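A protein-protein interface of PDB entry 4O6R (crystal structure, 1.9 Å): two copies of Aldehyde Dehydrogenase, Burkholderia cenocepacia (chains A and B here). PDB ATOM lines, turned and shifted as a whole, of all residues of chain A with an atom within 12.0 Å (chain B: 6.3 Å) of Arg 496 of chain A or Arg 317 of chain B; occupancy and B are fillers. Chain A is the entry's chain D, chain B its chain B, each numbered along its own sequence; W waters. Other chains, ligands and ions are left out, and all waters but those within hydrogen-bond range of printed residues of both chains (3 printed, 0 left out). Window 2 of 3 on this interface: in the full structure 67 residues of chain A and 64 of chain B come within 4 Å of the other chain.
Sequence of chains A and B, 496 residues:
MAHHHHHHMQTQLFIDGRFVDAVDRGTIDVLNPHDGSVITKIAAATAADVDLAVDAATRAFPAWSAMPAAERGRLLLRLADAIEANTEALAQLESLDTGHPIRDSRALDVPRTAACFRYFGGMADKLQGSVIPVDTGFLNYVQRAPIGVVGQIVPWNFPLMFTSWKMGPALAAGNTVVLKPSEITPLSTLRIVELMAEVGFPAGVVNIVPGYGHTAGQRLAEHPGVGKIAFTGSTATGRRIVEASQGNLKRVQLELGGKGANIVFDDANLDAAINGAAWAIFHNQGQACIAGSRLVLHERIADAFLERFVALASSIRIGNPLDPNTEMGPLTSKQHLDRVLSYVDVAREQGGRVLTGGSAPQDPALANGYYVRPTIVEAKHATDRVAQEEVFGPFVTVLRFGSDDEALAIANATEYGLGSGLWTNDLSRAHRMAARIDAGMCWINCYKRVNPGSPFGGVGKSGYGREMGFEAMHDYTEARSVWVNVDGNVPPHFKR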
ATOM      1  N   VAL A 490      -9.906  11.982  36.904  1.00  0.00           N
ATOM      2  CA  VAL A 490      -9.391  11.385  35.660  1.00  0.00           C
ATOM      3  C   VAL A 490     -10.482  11.205  34.610  1.00  0.00           C
ATOM      4  O   VAL A 490     -11.426  10.467  34.842  1.00  0.00           O
ATOM      5  CB  VAL A 490      -8.817   9.990  35.960  1.00  0.00           C
ATOM      6  CG1 VAL A 490      -8.176   9.390  34.709  1.00  0.00           C
ATOM      7  CG2 VAL A 490      -7.787  10.076  37.087  1.00  0.00           C
ATOM      8  N   PRO A 491     -10.360  11.865  33.448  1.00  0.00           N
ATOM      9  CA  PRO A 491     -11.422  11.666  32.447  1.00  0.00           C
ATOM     10  C   PRO A 491     -11.410  10.252  31.886  1.00  0.00           C
ATOM     11  O   PRO A 491     -10.360   9.625  31.825  1.00  0.00           O
ATOM     12  CB  PRO A 491     -11.084  12.659  31.327  1.00  0.00           C
ATOM     13  CG  PRO A 491      -9.955  13.486  31.817  1.00  0.00           C
ATOM     14  CD  PRO A 491      -9.315  12.789  32.980  1.00  0.00           C
ATOM     15  N   PRO A 492     -12.577   9.746  31.491  1.00  0.00           N
ATOM     16  CA  PRO A 492     -12.611   8.435  30.851  1.00  0.00           C
ATOM     17  C   PRO A 492     -11.723   8.411  29.624  1.00  0.00           C
ATOM     18  O   PRO A 492     -11.697   9.389  28.882  1.00  0.00           O
ATOM     19  CB  PRO A 492     -14.080   8.282  30.445  1.00  0.00           C
ATOM     20  CG  PRO A 492     -14.811   9.127  31.428  1.00  0.00           C
ATOM     21  CD  PRO A 492     -13.922  10.330  31.597  1.00  0.00           C
ATOM     22  N   HIS A 493     -11.003   7.304  29.444  1.00  0.00           N
ATOM     23  CA  HIS A 493     -10.127   7.105  28.305  1.00  0.00           C
ATOM     24  C   HIS A 493     -10.936   6.828  27.048  1.00  0.00           C
ATOM     25  O   HIS A 493     -10.557   7.305  25.956  1.00  0.00           O
ATOM     26  CB  HIS A 493      -9.166   5.940  28.569  1.00  0.00           C
ATOM     27  CG  HIS A 493      -8.199   5.696  27.459  1.00  0.00           C
ATOM     28  ND1 HIS A 493      -7.191   6.575  27.148  1.00  0.00           N
ATOM     29  CD2 HIS A 493      -8.106   4.691  26.565  1.00  0.00           C
ATOM     30  CE1 HIS A 493      -6.516   6.126  26.108  1.00  0.00           C
ATOM     31  NE2 HIS A 493      -7.053   4.984  25.735  1.00  0.00           N
ATOM     32  N   PHE A 494     -12.018   6.050  27.200  1.00  0.00           N
ATOM     33  CA  PHE A 494     -12.992   5.802  26.137  1.00  0.00           C
ATOM     34  C   PHE A 494     -14.247   6.639  26.410  1.00  0.00           C
ATOM     35  O   PHE A 494     -15.108   6.247  27.209  1.00  0.00           O
ATOM     36  CB  PHE A 494     -13.332   4.307  26.048  1.00  0.00           C
ATOM     37  CG  PHE A 494     -12.120   3.423  25.944  1.00  0.00           C
ATOM     38  CD1 PHE A 494     -11.454   3.298  24.753  1.00  0.00           C
ATOM     39  CD2 PHE A 494     -11.627   2.748  27.048  1.00  0.00           C
ATOM     40  CE1 PHE A 494     -10.314   2.520  24.639  1.00  0.00           C
ATOM     41  CE2 PHE A 494     -10.479   1.959  26.949  1.00  0.00           C
ATOM     42  CZ  PHE A 494      -9.833   1.841  25.741  1.00  0.00           C
ATOM     43  N   LYS A 495     -14.319   7.790  25.755  1.00  0.00           N
ATOM     44  CA  LYS A 495     -15.360   8.787  26.017  1.00  0.00           C
ATOM     45  C   LYS A 495     -16.707   8.379  25.451  1.00  0.00           C
ATOM     46  O   LYS A 495     -16.840   8.101  24.244  1.00  0.00           O
ATOM     47  CB  LYS A 495     -14.954  10.153  25.457  1.00  0.00           C
ATOM     48  CG  LYS A 495     -13.598  10.582  25.998  1.00  0.00           C
ATOM     49  CD  LYS A 495     -13.271  12.041  25.727  1.00  0.00           C
ATOM     50  CE  LYS A 495     -11.834  12.338  26.080  1.00  0.00           C
ATOM     51  NZ  LYS A 495     -11.594  12.146  27.552  1.00  0.00           N
ATOM     52  N   ARG A 496     -17.708   8.351  26.321  1.00  0.00           N
ATOM     53  CA  ARG A 496     -19.054   7.966  25.917  1.00  0.00           C
ATOM     54  C   ARG A 496     -20.092   8.968  26.418  1.00  0.00           C
ATOM     55  O   ARG A 496     -19.789   9.861  27.204  1.00  0.00           O
ATOM     56  CB  ARG A 496     -19.397   6.571  26.445  1.00  0.00           C
ATOM     57  CG  ARG A 496     -18.480   5.470  25.914  1.00  0.00           C
ATOM     58  CD  ARG A 496     -18.672   5.280  24.401  1.00  0.00           C
ATOM     59  NE  ARG A 496     -17.883   4.193  23.875  1.00  0.00           N
ATOM     60  CZ  ARG A 496     -16.623   4.304  23.442  1.00  0.00           C
ATOM     61  NH1 ARG A 496     -15.987   5.468  23.475  1.00  0.00           N
ATOM     62  NH2 ARG A 496     -16.001   3.233  22.987  1.00  0.00           N
ATOM     63  OXT ARG A 496     -21.245   8.882  26.014  1.00  0.00           O
ATOM     64  N   ARG B 103      -3.978   8.906  18.635  1.00  0.00           N
ATOM     65  CA  ARG B 103      -4.454   9.728  19.712  1.00  0.00           C
ATOM     66  C   ARG B 103      -3.634   9.431  20.987  1.00  0.00           C
ATOM     67  O   ARG B 103      -3.396  10.330  21.785  1.00  0.00           O
ATOM     68  CB  ARG B 103      -5.962   9.547  19.916  1.00  0.00           C
ATOM     69  CG  ARG B 103      -6.374   8.235  20.518  1.00  0.00           C
ATOM     70  CD  ARG B 103      -7.873   8.235  20.745  1.00  0.00           C
ATOM     71  NE  ARG B 103      -8.181   7.366  21.865  1.00  0.00           N
ATOM     72  CZ  ARG B 103      -9.330   7.366  22.534  1.00  0.00           C
ATOM     73  NH1 ARG B 103     -10.339   8.164  22.154  1.00  0.00           N
ATOM     74  NH2 ARG B 103      -9.475   6.546  23.561  1.00  0.00           N
ATOM     75  N   LEU B 312     -19.143  -1.434  27.357  1.00  0.00           N
ATOM     76  CA  LEU B 312     -18.085  -0.497  27.020  1.00  0.00           C
ATOM     77  C   LEU B 312     -17.023  -1.135  26.107  1.00  0.00           C
ATOM     78  O   LEU B 312     -16.671  -0.597  25.040  1.00  0.00           O
ATOM     79  CB  LEU B 312     -17.457   0.096  28.296  1.00  0.00           C
ATOM     80  CG  LEU B 312     -16.250   1.022  28.105  1.00  0.00           C
ATOM     81  CD1 LEU B 312     -16.622   2.116  27.136  1.00  0.00           C
ATOM     82  CD2 LEU B 312     -15.786   1.648  29.422  1.00  0.00           C
ATOM     83  N   ALA B 313     -16.542  -2.292  26.518  1.00  0.00           N
ATOM     84  CA  ALA B 313     -15.506  -2.989  25.778  1.00  0.00           C
ATOM     85  C   ALA B 313     -15.902  -3.304  24.337  1.00  0.00           C
ATOM     86  O   ALA B 313     -15.094  -3.123  23.417  1.00  0.00           O
ATOM     87  CB  ALA B 313     -15.113  -4.268  26.502  1.00  0.00           C
ATOM     88  N   SER B 314     -17.143  -3.772  24.142  1.00  0.00           N
ATOM     89  CA  SER B 314     -17.629  -4.124  22.815  1.00  0.00           C
ATOM     90  C   SER B 314     -17.734  -2.892  21.927  1.00  0.00           C
ATOM     91  O   SER B 314     -17.690  -3.000  20.720  1.00  0.00           O
ATOM     92  CB  SER B 314     -19.000  -4.803  22.893  1.00  0.00           C
ATOM     93  OG  SER B 314     -18.955  -5.936  23.730  1.00  0.00           O
ATOM     94  N   SER B 315     -17.897  -1.723  22.526  1.00  0.00           N
ATOM     95  CA  SER B 315     -18.018  -0.474  21.757  1.00  0.00           C
ATOM     96  C   SER B 315     -16.674   0.144  21.340  1.00  0.00           C
ATOM     97  O   SER B 315     -16.647   1.063  20.565  1.00  0.00           O
ATOM     98  CB  SER B 315     -18.831   0.559  22.564  1.00  0.00           C
ATOM     99  OG  SER B 315     -18.039   1.126  23.596  1.00  0.00           O
ATOM    100  N   ILE B 316     -15.568  -0.312  21.916  1.00  0.00           N
ATOM    101  CA  ILE B 316     -14.263   0.300  21.657  1.00  0.00           C
ATOM    102  C   ILE B 316     -13.977   0.269  20.163  1.00  0.00           C
ATOM    103  O   ILE B 316     -14.126  -0.763  19.515  1.00  0.00           O
ATOM    104  CB  ILE B 316     -13.154  -0.419  22.438  1.00  0.00           C
ATOM    105  CG1 ILE B 316     -13.286  -0.100  23.939  1.00  0.00           C
ATOM    106  CG2 ILE B 316     -11.741  -0.059  21.912  1.00  0.00           C
ATOM    107  CD1 ILE B 316     -12.248  -0.781  24.821  1.00  0.00           C
ATOM    108  N   ARG B 317     -13.555   1.399  19.612  1.00  0.00           N
ATOM    109  CA  ARG B 317     -13.383   1.527  18.158  1.00  0.00           C
ATOM    110  C   ARG B 317     -11.986   1.039  17.788  1.00  0.00           C
ATOM    111  O   ARG B 317     -10.950   1.692  18.093  1.00  0.00           O
ATOM    112  CB  ARG B 317     -13.588   2.961  17.729  1.00  0.00           C
ATOM    113  CG  ARG B 317     -14.957   3.528  18.145  1.00  0.00           C
ATOM    114  CD  ARG B 317     -15.180   4.913  17.554  1.00  0.00           C
ATOM    115  NE  ARG B 317     -14.213   5.911  18.039  1.00  0.00           N
ATOM    116  CZ  ARG B 317     -14.415   6.714  19.084  1.00  0.00           C
ATOM    117  NH1 ARG B 317     -15.541   6.634  19.794  1.00  0.00           N
ATOM    118  NH2 ARG B 317     -13.489   7.591  19.427  1.00  0.00           N
ATOM    119  N   ILE B 318     -11.970  -0.098  17.118  1.00  0.00           N
ATOM    120  CA  ILE B 318     -10.747  -0.760  16.672  1.00  0.00           C
ATOM    121  C   ILE B 318     -10.483  -0.351  15.238  1.00  0.00           C
ATOM    122  O   ILE B 318     -11.390  -0.360  14.407  1.00  0.00           O
ATOM    123  CB  ILE B 318     -10.883  -2.290  16.665  1.00  0.00           C
ATOM    124  CG1 ILE B 318     -11.403  -2.807  18.004  1.00  0.00           C
ATOM    125  CG2 ILE B 318      -9.549  -2.939  16.306  1.00  0.00           C
ATOM    126  CD1 ILE B 318     -12.159  -4.124  17.903  1.00  0.00           C
ATOM    127  N   GLY B 319      -9.251  -0.007  14.929  1.00  0.00           N
ATOM    128  CA  GLY B 319      -8.974   0.405  13.566  1.00  0.00           C
ATOM    129  C   GLY B 319      -7.588   0.908  13.333  1.00  0.00           C
ATOM    130  O   GLY B 319      -6.714   0.750  14.178  1.00  0.00           O
ATOM    131  N   PRO B 324      -7.615   9.315  13.773  1.00  0.00           N
ATOM    132  CA  PRO B 324      -7.757   9.902  15.105  1.00  0.00           C
ATOM    133  C   PRO B 324      -8.970   9.387  15.904  1.00  0.00           C
ATOM    134  O   PRO B 324      -9.017   9.577  17.125  1.00  0.00           O
ATOM    135  CB  PRO B 324      -7.893  11.395  14.817  1.00  0.00           C
ATOM    136  CG  PRO B 324      -8.496  11.454  13.450  1.00  0.00           C
ATOM    137  CD  PRO B 324      -7.844  10.314  12.713  1.00  0.00           C
ATOM    138  N   ASN B 325      -9.928   8.742  15.230  1.00  0.00           N
ATOM    139  CA  ASN B 325     -11.097   8.147  15.899  1.00  0.00           C
ATOM    140  C   ASN B 325     -10.824   6.751  16.457  1.00  0.00           C
ATOM    141  O   ASN B 325     -11.654   6.208  17.173  1.00  0.00           O
ATOM    142  CB  ASN B 325     -12.233   8.038  14.915  1.00  0.00           C
ATOM    143  CG  ASN B 325     -12.646   9.385  14.391  1.00  0.00           C
ATOM    144  OD1 ASN B 325     -13.236  10.193  15.125  1.00  0.00           O
ATOM    145  ND2 ASN B 325     -12.310   9.662  13.127  1.00  0.00           N
ATOM    146  N   THR B 326      -9.672   6.165  16.098  1.00  0.00           N
ATOM    147  CA  THR B 326      -9.327   4.830  16.561  1.00  0.00           C
ATOM    148  C   THR B 326      -8.999   4.880  18.031  1.00  0.00           C
ATOM    149  O   THR B 326      -8.185   5.714  18.480  1.00  0.00           O
ATOM    150  CB  THR B 326      -8.151   4.236  15.762  1.00  0.00           C
ATOM    151  OG1 THR B 326      -8.592   3.963  14.431  1.00  0.00           O
ATOM    152  CG2 THR B 326      -7.625   2.952  16.411  1.00  0.00           C
ATOM    153  N   GLU B 327      -9.651   4.005  18.783  1.00  0.00           N
ATOM    154  CA  GLU B 327      -9.417   3.868  20.210  1.00  0.00           C
ATOM    155  C   GLU B 327      -8.501   2.692  20.546  1.00  0.00           C
ATOM    156  O   GLU B 327      -7.840   2.682  21.588  1.00  0.00           O
ATOM    157  CB  GLU B 327     -10.729   3.703  20.943  1.00  0.00           C
ATOM    158  CG  GLU B 327     -11.619   4.936  20.927  1.00  0.00           C
ATOM    159  CD  GLU B 327     -12.952   4.689  21.625  1.00  0.00           C
ATOM    160  OE1 GLU B 327     -13.558   3.600  21.394  1.00  0.00           O
ATOM    161  OE2 GLU B 327     -13.372   5.586  22.415  1.00  0.00           O
ATOM    162  N   MET B 328      -8.455   1.700  19.677  1.00  0.00           N
ATOM    163  CA  MET B 328      -7.608   0.556  19.906  1.00  0.00           C
ATOM    164  C   MET B 328      -7.029   0.126  18.583  1.00  0.00           C
ATOM    165  O   MET B 328      -7.750   0.022  17.594  1.00  0.00           O
ATOM    166  CB  MET B 328      -8.367  -0.604  20.602  1.00  0.00           C
ATOM    167  CG  MET B 328      -7.702  -1.983  20.423  1.00  0.00           C
ATOM    168  SD  MET B 328      -8.262  -3.387  21.484  1.00  0.00           S
ATOM    169  CE  MET B 328      -7.980  -2.660  23.025  1.00  0.00           C
ATOM    170  N   GLY B 329      -5.712  -0.073  18.581  1.00  0.00           N
ATOM    171  CA  GLY B 329      -4.956  -0.480  17.397  1.00  0.00           C
ATOM    172  C   GLY B 329      -4.742  -1.978  17.335  1.00  0.00           C
ATOM    173  O   GLY B 329      -5.287  -2.749  18.146  1.00  0.00           O
HETATM  174  O   HOH W   1     -15.726   8.790  21.821  1.00  0.00           O
HETATM  175  O   HOH W   2      -7.057   5.002  22.825  1.00  0.00           O
HETATM  176  O   HOH W   3     -12.674   7.981  23.378  1.00  0.00           O
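The backbone carbonyl oxygen of His 493 of chain A is in hydrogen-bond range of the guanidinium group of Arg 103 of chain B, at 2.7 Å. The side-chain hydroxyl (OG) of Ser 315 of chain B sits at hydrogen-bond distance from the guanidinium group (NH2) of Arg 496 of chain A, 3.0 Å away. NH1 of Arg 496 of chain A is in salt-bridge range of OE2 of Glu 327 of chain B, 2.8 Å away.
OE2 of Glu 327 of chain B is in salt-bridge range of NH1 of Arg 103 of chain B. The backbone carbonyl oxygen (O) of Leu 312 of chain B sits at hydrogen-bond distance from the side-chain hydroxyl (OG) of Ser 315 of chain B (2.6 Å). NE of Arg 317 of chain B lies within hydrogen-bond range of O of Asn 325 of chain B, at 2.7 Å. The guanidinium group (NH1) of Arg 317 of chain B is in salt-bridge range of the side-chain carboxylate (OE2) of Glu 327 of chain B (3.6 Å). O of Arg 317 of chain B is in hydrogen-bond range of N of Met 328 of chain B (3.0 Å).
Phe 494 of chain A touches Arg 103 of chain B. CZ of Phe 494 of chain A touches CD1 of Ile 316 of chain B, at 3.7 Å. CD1 of Phe 494 of chain A touches CD of Glu 327 of chain B (3.7 Å). Ile 316 of chain B touches Arg 496 of chain A. Arg 317 of chain B touches Arg 496 of chain A (NH1 to NH1, 3.9 Å).
Arg 496 of chain A touches just these residues of chain B: Ser 315 (3.0 Å), Ile 316 (3.7 Å), Arg 317 (3.9 Å) and Glu 327 (2.8 Å). Arg 317 of chain B touches one residue of chain A. Ser 315 of chain B touches one residue of chain A. Of chain A, only Phe 494 (3.7 Å) and Arg 496 (3.7 Å) come within 4 Å of Ile 316 of chain B. No residue of chain A comes within 4 Å of Gly 319 of chain B. No residue of chain A comes within 4 Å of Asn 325 of chain B. Of chain A, only Phe 494 (3.7 Å) and Arg 496 (2.8 Å) come within 4 Å of Glu 327 of chain B. No residue of chain A comes within 4 Å of Met 328 of chain B. Gly 329 of chain B touches none of the printed residues of chain A. Of the printed residues of chain B, Phe 494 of chain A touches Arg 103 (3.99 Å), Ile 316 (3.7 Å) and Glu 327 (3.7 Å). Printed residues of chain A within 4 Å of Arg 103 of chain B: His 493 (2.7 Å) and Phe 494 (3.99 Å). Printed residues of chain B within 4 Å of His 493 of chain A: Arg 103.
Among the printed residues, 8 pairs touch across the chains.
No position is printed for both chains. Of the 8 pairs that touch across the chains among the printed residues, none has its exchanged pair printed and touching as well.
Water W3 lies within hydrogen-bond range of the guanidinium group (NH1) of Arg 103 of chain B, the side-chain carboxylate (OE2) of Glu 327 of chain B, the backbone NH (N) of Lys 495 of chain A and the backbone carbonyl oxygen (O) of His 493 of chain A. Water W2 lies within hydrogen-bond range of the backbone carbonyl oxygen (O) of Glu 327 of chain B (2.7 Å), the guanidinium group (NE) of Arg 103 of chain B (2.8 Å) and a ring nitrogen (NE2) of His 493 of chain A (2.9 Å). Water W1 lies within hydrogen-bond range of the backbone carbonyl oxygen (O) of Lys 495 of chain A and the guanidinium group (NH1) of Arg 317 of chain B.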
